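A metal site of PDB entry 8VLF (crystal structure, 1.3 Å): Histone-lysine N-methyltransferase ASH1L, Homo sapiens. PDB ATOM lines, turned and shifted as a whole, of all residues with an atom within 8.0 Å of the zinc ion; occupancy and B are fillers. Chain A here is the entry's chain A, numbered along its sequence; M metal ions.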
ATOM      1  N   ILE A   6      23.059  17.139  -8.481  1.00  0.00           N
ATOM      2  CA  ILE A   6      21.788  16.442  -8.408  1.00  0.00           C
ATOM      3  C   ILE A   6      20.684  17.497  -8.491  1.00  0.00           C
ATOM      4  O   ILE A   6      20.647  18.423  -7.672  1.00  0.00           O
ATOM      5  CB  ILE A   6      21.667  15.619  -7.107  1.00  0.00           C
ATOM      6  CG1 ILE A   6      22.741  14.523  -7.079  1.00  0.00           C
ATOM      7  CG2 ILE A   6      20.280  15.007  -6.986  1.00  0.00           C
ATOM      8  CD1 ILE A   6      22.753  13.700  -5.811  1.00  0.00           C
ATOM      9  N   ARG A   7      19.801  17.378  -9.472  1.00  0.00           N
ATOM     10  CA  ARG A   7      18.651  18.289  -9.538  1.00  0.00           C
ATOM     11  C   ARG A   7      17.478  17.483 -10.090  1.00  0.00           C
ATOM     12  O   ARG A   7      17.237  17.472 -11.292  1.00  0.00           O
ATOM     13  CB  ARG A   7      18.901  19.525 -10.387  1.00  0.00           C
ATOM     14  CG  ARG A   7      17.785  20.546 -10.176  1.00  0.00           C
ATOM     15  CD  ARG A   7      17.655  21.547 -11.300  1.00  0.00           C
ATOM     16  NE  ARG A   7      17.345  20.916 -12.582  1.00  0.00           N
ATOM     17  CZ  ARG A   7      16.166  20.391 -12.916  1.00  0.00           C
ATOM     18  NH1 ARG A   7      15.150  20.392 -12.054  1.00  0.00           N
ATOM     19  NH2 ARG A   7      15.997  19.851 -14.122  1.00  0.00           N
ATOM     20  N   CYS A   8      16.764  16.814  -9.197  1.00  0.00           N
ATOM     21  CA  CYS A   8      15.632  15.989  -9.573  1.00  0.00           C
ATOM     22  C   CYS A   8      14.342  16.738  -9.274  1.00  0.00           C
ATOM     23  O   CYS A   8      14.324  17.704  -8.511  1.00  0.00           O
ATOM     24  CB  CYS A   8      15.690  14.674  -8.797  1.00  0.00           C
ATOM     25  SG  CYS A   8      14.517  13.468  -9.363  1.00  0.00           S
ATOM     26  N   ILE A   9      13.247  16.261  -9.874  1.00  0.00           N
ATOM     27  CA  ILE A   9      11.961  16.902  -9.609  1.00  0.00           C
ATOM     28  C   ILE A   9      11.547  16.758  -8.145  1.00  0.00           C
ATOM     29  O   ILE A   9      10.752  17.561  -7.647  1.00  0.00           O
ATOM     30  CB  ILE A   9      10.839  16.395 -10.535  1.00  0.00           C
ATOM     31  CG1 ILE A   9      10.570  14.898 -10.308  1.00  0.00           C
ATOM     32  CG2 ILE A   9      11.168  16.712 -11.989  1.00  0.00           C
ATOM     33  CD1 ILE A   9       9.469  14.347 -11.182  1.00  0.00           C
ATOM     34  N   CYS A  10      12.065  15.735  -7.450  1.00  0.00           N
ATOM     35  CA  CYS A  10      11.731  15.572  -6.032  1.00  0.00           C
ATOM     36  C   CYS A  10      12.370  16.646  -5.148  1.00  0.00           C
ATOM     37  O   CYS A  10      11.904  16.843  -4.030  1.00  0.00           O
ATOM     38  CB  CYS A  10      12.121  14.174  -5.536  1.00  0.00           C
ATOM     39  SG  CYS A  10      13.926  13.919  -5.560  1.00  0.00           S
ATOM     40  N   GLY A  11      13.419  17.322  -5.619  1.00  0.00           N
ATOM     41  CA  GLY A  11      14.029  18.377  -4.822  1.00  0.00           C
ATOM     42  C   GLY A  11      14.888  17.890  -3.680  1.00  0.00           C
ATOM     43  O   GLY A  11      15.341  18.707  -2.878  1.00  0.00           O
ATOM     44  N   LEU A  12      15.117  16.575  -3.569  1.00  0.00           N
ATOM     45  CA  LEU A  12      15.972  16.029  -2.528  1.00  0.00           C
ATOM     46  C   LEU A  12      17.365  15.833  -3.099  1.00  0.00           C
ATOM     47  O   LEU A  12      17.531  15.145  -4.117  1.00  0.00           O
ATOM     48  CB  LEU A  12      15.421  14.700  -2.010  1.00  0.00           C
ATOM     49  CG  LEU A  12      14.159  14.836  -1.166  1.00  0.00           C
ATOM     50  CD1 LEU A  12      13.594  13.467  -0.813  1.00  0.00           C
ATOM     51  CD2 LEU A  12      14.422  15.649   0.105  1.00  0.00           C
ATOM     52  N   TYR A  13      18.357  16.424  -2.444  1.00  0.00           N
ATOM     53  CA  TYR A  13      19.757  16.322  -2.870  1.00  0.00           C
ATOM     54  C   TYR A  13      20.323  15.046  -2.272  1.00  0.00           C
ATOM     55  O   TYR A  13      21.071  15.041  -1.300  1.00  0.00           O
ATOM     56  CB  TYR A  13      20.562  17.559  -2.447  1.00  0.00           C
ATOM     57  CG  TYR A  13      21.743  17.763  -3.365  1.00  0.00           C
ATOM     58  CD1 TYR A  13      22.900  16.987  -3.237  1.00  0.00           C
ATOM     59  CD2 TYR A  13      21.698  18.692  -4.399  1.00  0.00           C
ATOM     60  CE1 TYR A  13      23.967  17.166  -4.095  1.00  0.00           C
ATOM     61  CE2 TYR A  13      22.768  18.875  -5.266  1.00  0.00           C
ATOM     62  CZ  TYR A  13      23.887  18.090  -5.118  1.00  0.00           C
ATOM     63  OH  TYR A  13      24.935  18.274  -5.990  1.00  0.00           O
ATOM     64  N   LYS A  14      19.942  13.925  -2.854  1.00  0.00           N
ATOM     65  CA  LYS A  14      20.461  12.660  -2.357  1.00  0.00           C
ATOM     66  C   LYS A  14      20.804  11.731  -3.501  1.00  0.00           C
ATOM     67  O   LYS A  14      20.072  11.625  -4.491  1.00  0.00           O
ATOM     68  CB  LYS A  14      19.558  11.970  -1.341  1.00  0.00           C
ATOM     69  CG  LYS A  14      18.243  11.500  -1.858  1.00  0.00           C
ATOM     70  CD  LYS A  14      17.502  10.880  -0.690  1.00  0.00           C
ATOM     71  CE  LYS A  14      16.184  10.360  -1.130  1.00  0.00           C
ATOM     72  NZ  LYS A  14      15.309   9.707  -0.109  1.00  0.00           N
ATOM     73  N   GLU A  16      20.735   8.291  -4.528  1.00  0.00           N
ATOM     74  CA  GLU A  16      20.012   7.083  -4.155  1.00  0.00           C
ATOM     75  C   GLU A  16      19.501   6.401  -5.414  1.00  0.00           C
ATOM     76  O   GLU A  16      18.962   7.064  -6.306  1.00  0.00           O
ATOM     77  CB  GLU A  16      18.830   7.369  -3.222  1.00  0.00           C
ATOM     78  CG  GLU A  16      17.829   6.212  -3.144  1.00  0.00           C
ATOM     79  CD  GLU A  16      16.460   6.641  -2.652  1.00  0.00           C
ATOM     80  OE1 GLU A  16      15.435   6.063  -3.089  1.00  0.00           O
ATOM     81  OE2 GLU A  16      16.409   7.519  -1.770  1.00  0.00           O
ATOM     82  N   LEU A  18      19.056   4.073  -8.913  1.00  0.00           N
ATOM     83  CA  LEU A  18      19.493   4.341 -10.270  1.00  0.00           C
ATOM     84  C   LEU A  18      19.231   5.810 -10.612  1.00  0.00           C
ATOM     85  O   LEU A  18      18.108   6.296 -10.476  1.00  0.00           O
ATOM     86  CB  LEU A  18      18.725   3.459 -11.240  1.00  0.00           C
ATOM     87  CG  LEU A  18      19.369   3.250 -12.618  1.00  0.00           C
ATOM     88  CD1 LEU A  18      20.863   2.883 -12.529  1.00  0.00           C
ATOM     89  CD2 LEU A  18      18.596   2.226 -13.408  1.00  0.00           C
ATOM     90  N   MET A  19      20.257   6.482 -11.080  1.00  0.00           N
ATOM     91  CA  MET A  19      20.153   7.885 -11.413  1.00  0.00           C
ATOM     92  C   MET A  19      20.612   8.055 -12.850  1.00  0.00           C
ATOM     93  O   MET A  19      21.413   7.265 -13.352  1.00  0.00           O
ATOM     94  CB  MET A  19      21.028   8.692 -10.442  1.00  0.00           C
ATOM     95  CG  MET A  19      20.482   8.664  -9.023  1.00  0.00           C
ATOM     96  SD  MET A  19      21.174   9.909  -7.928  1.00  0.00           S
ATOM     97  CE  MET A  19      20.349  11.389  -8.501  1.00  0.00           C
ATOM     98  N   TRP A  28      21.854  15.305 -12.557  1.00  0.00           N
ATOM     99  CA  TRP A  28      21.456  13.935 -12.298  1.00  0.00           C
ATOM    100  C   TRP A  28      20.067  13.909 -11.645  1.00  0.00           C
ATOM    101  O   TRP A  28      19.764  14.743 -10.774  1.00  0.00           O
ATOM    102  CB  TRP A  28      22.464  13.261 -11.364  1.00  0.00           C
ATOM    103  CG  TRP A  28      23.791  13.038 -12.003  1.00  0.00           C
ATOM    104  CD1 TRP A  28      24.845  13.913 -12.041  1.00  0.00           C
ATOM    105  CD2 TRP A  28      24.211  11.874 -12.725  1.00  0.00           C
ATOM    106  NE1 TRP A  28      25.895  13.358 -12.722  1.00  0.00           N
ATOM    107  CE2 TRP A  28      25.536  12.105 -13.159  1.00  0.00           C
ATOM    108  CE3 TRP A  28      23.606  10.644 -13.043  1.00  0.00           C
ATOM    109  CZ2 TRP A  28      26.249  11.162 -13.893  1.00  0.00           C
ATOM    110  CZ3 TRP A  28      24.317   9.721 -13.768  1.00  0.00           C
ATOM    111  CH2 TRP A  28      25.632   9.979 -14.177  1.00  0.00           C
ATOM    112  N   GLN A  29      19.254  12.958 -12.070  1.00  0.00           N
ATOM    113  CA  GLN A  29      17.899  12.809 -11.566  1.00  0.00           C
ATOM    114  C   GLN A  29      17.666  11.349 -11.205  1.00  0.00           C
ATOM    115  O   GLN A  29      18.338  10.447 -11.719  1.00  0.00           O
ATOM    116  CB  GLN A  29      16.893  13.269 -12.624  1.00  0.00           C
ATOM    117  CG  GLN A  29      17.219  14.634 -13.196  1.00  0.00           C
ATOM    118  CD  GLN A  29      16.036  15.301 -13.879  1.00  0.00           C
ATOM    119  OE1 GLN A  29      15.531  14.787 -14.873  1.00  0.00           O
ATOM    120  NE2 GLN A  29      15.569  16.427 -13.341  1.00  0.00           N
ATOM    121  N   HIS A  30      16.720  11.103 -10.290  1.00  0.00           N
ATOM    122  CA  HIS A  30      16.394   9.726  -9.933  1.00  0.00           C
ATOM    123  C   HIS A  30      15.510   9.131 -11.028  1.00  0.00           C
ATOM    124  O   HIS A  30      14.472   9.701 -11.372  1.00  0.00           O
ATOM    125  CB  HIS A  30      15.665   9.660  -8.585  1.00  0.00           C
ATOM    126  CG  HIS A  30      16.397  10.356  -7.479  1.00  0.00           C
ATOM    127  ND1 HIS A  30      15.935  11.519  -6.885  1.00  0.00           N
ATOM    128  CD2 HIS A  30      17.576  10.074  -6.873  1.00  0.00           C
ATOM    129  CE1 HIS A  30      16.792  11.908  -5.965  1.00  0.00           C
ATOM    130  NE2 HIS A  30      17.798  11.042  -5.927  1.00  0.00           N
ATOM    131  N   CYS A  31      15.906   7.972 -11.545  1.00  0.00           N
ATOM    132  CA  CYS A  31      15.106   7.322 -12.575  1.00  0.00           C
ATOM    133  C   CYS A  31      13.672   7.096 -12.111  1.00  0.00           C
ATOM    134  O   CYS A  31      12.723   7.296 -12.871  1.00  0.00           O
ATOM    135  CB  CYS A  31      15.746   6.007 -13.003  1.00  0.00           C
ATOM    136  SG  CYS A  31      17.298   6.226 -13.869  1.00  0.00           S
ATOM    137  N   ASP A  32      13.487   6.678 -10.857  1.00  0.00           N
ATOM    138  CA  ASP A  32      12.137   6.419 -10.364  1.00  0.00           C
ATOM    139  C   ASP A  32      11.282   7.683 -10.314  1.00  0.00           C
ATOM    140  O   ASP A  32      10.088   7.644 -10.616  1.00  0.00           O
ATOM    141  CB  ASP A  32      12.190   5.761  -8.986  1.00  0.00           C
ATOM    142  CG  ASP A  32      12.700   4.332  -9.033  1.00  0.00           C
ATOM    143  OD1 ASP A  32      12.742   3.750 -10.145  1.00  0.00           O
ATOM    144  OD2 ASP A  32      13.041   3.797  -7.965  1.00  0.00           O
ATOM    145  N   CYS A  33      11.884   8.815  -9.921  1.00  0.00           N
ATOM    146  CA  CYS A  33      11.119  10.057  -9.880  1.00  0.00           C
ATOM    147  C   CYS A  33      10.717  10.490 -11.276  1.00  0.00           C
ATOM    148  O   CYS A  33       9.636  11.048 -11.475  1.00  0.00           O
ATOM    149  CB  CYS A  33      11.952  11.176  -9.257  1.00  0.00           C
ATOM    150  SG  CYS A  33      12.384  10.966  -7.537  1.00  0.00           S
ATOM    151  N   MET A  34      11.582  10.232 -12.246  1.00  0.00           N
ATOM    152  CA  MET A  34      11.343  10.709 -13.608  1.00  0.00           C
ATOM    153  C   MET A  34      10.623   9.698 -14.493  1.00  0.00           C
ATOM    154  O   MET A  34      10.273  10.044 -15.618  1.00  0.00           O
ATOM    155  CB  MET A  34      12.653  11.130 -14.283  1.00  0.00           C
ATOM    156  CG  MET A  34      13.501  12.147 -13.534  1.00  0.00           C
ATOM    157  SD  MET A  34      12.582  13.604 -12.991  1.00  0.00           S
ATOM    158  CE  MET A  34      12.225  14.382 -14.575  1.00  0.00           C
HETATM  159 ZN    ZN M   1      14.120  12.431  -7.308  1.00  0.00          ZN
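NE2 of His 30 is in hydrogen-bond range of O of Lys 14 (2.8 Å).
N of Leu 12 sits close to SG of Cys 10, 3.5 Å away.
The zinc ion is bound by a ring nitrogen (ND1) of His 30, the side-chain sulfur (SG) of Cys 33, the side-chain sulfur (SG) of Cys 10 and the side-chain sulfur (SG) of Cys 8.
The zinc ion has four donor atoms within binding distance.
Within 4 Å of the zinc ion: Cys 8, Cys 10, His 30 and Cys 33.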
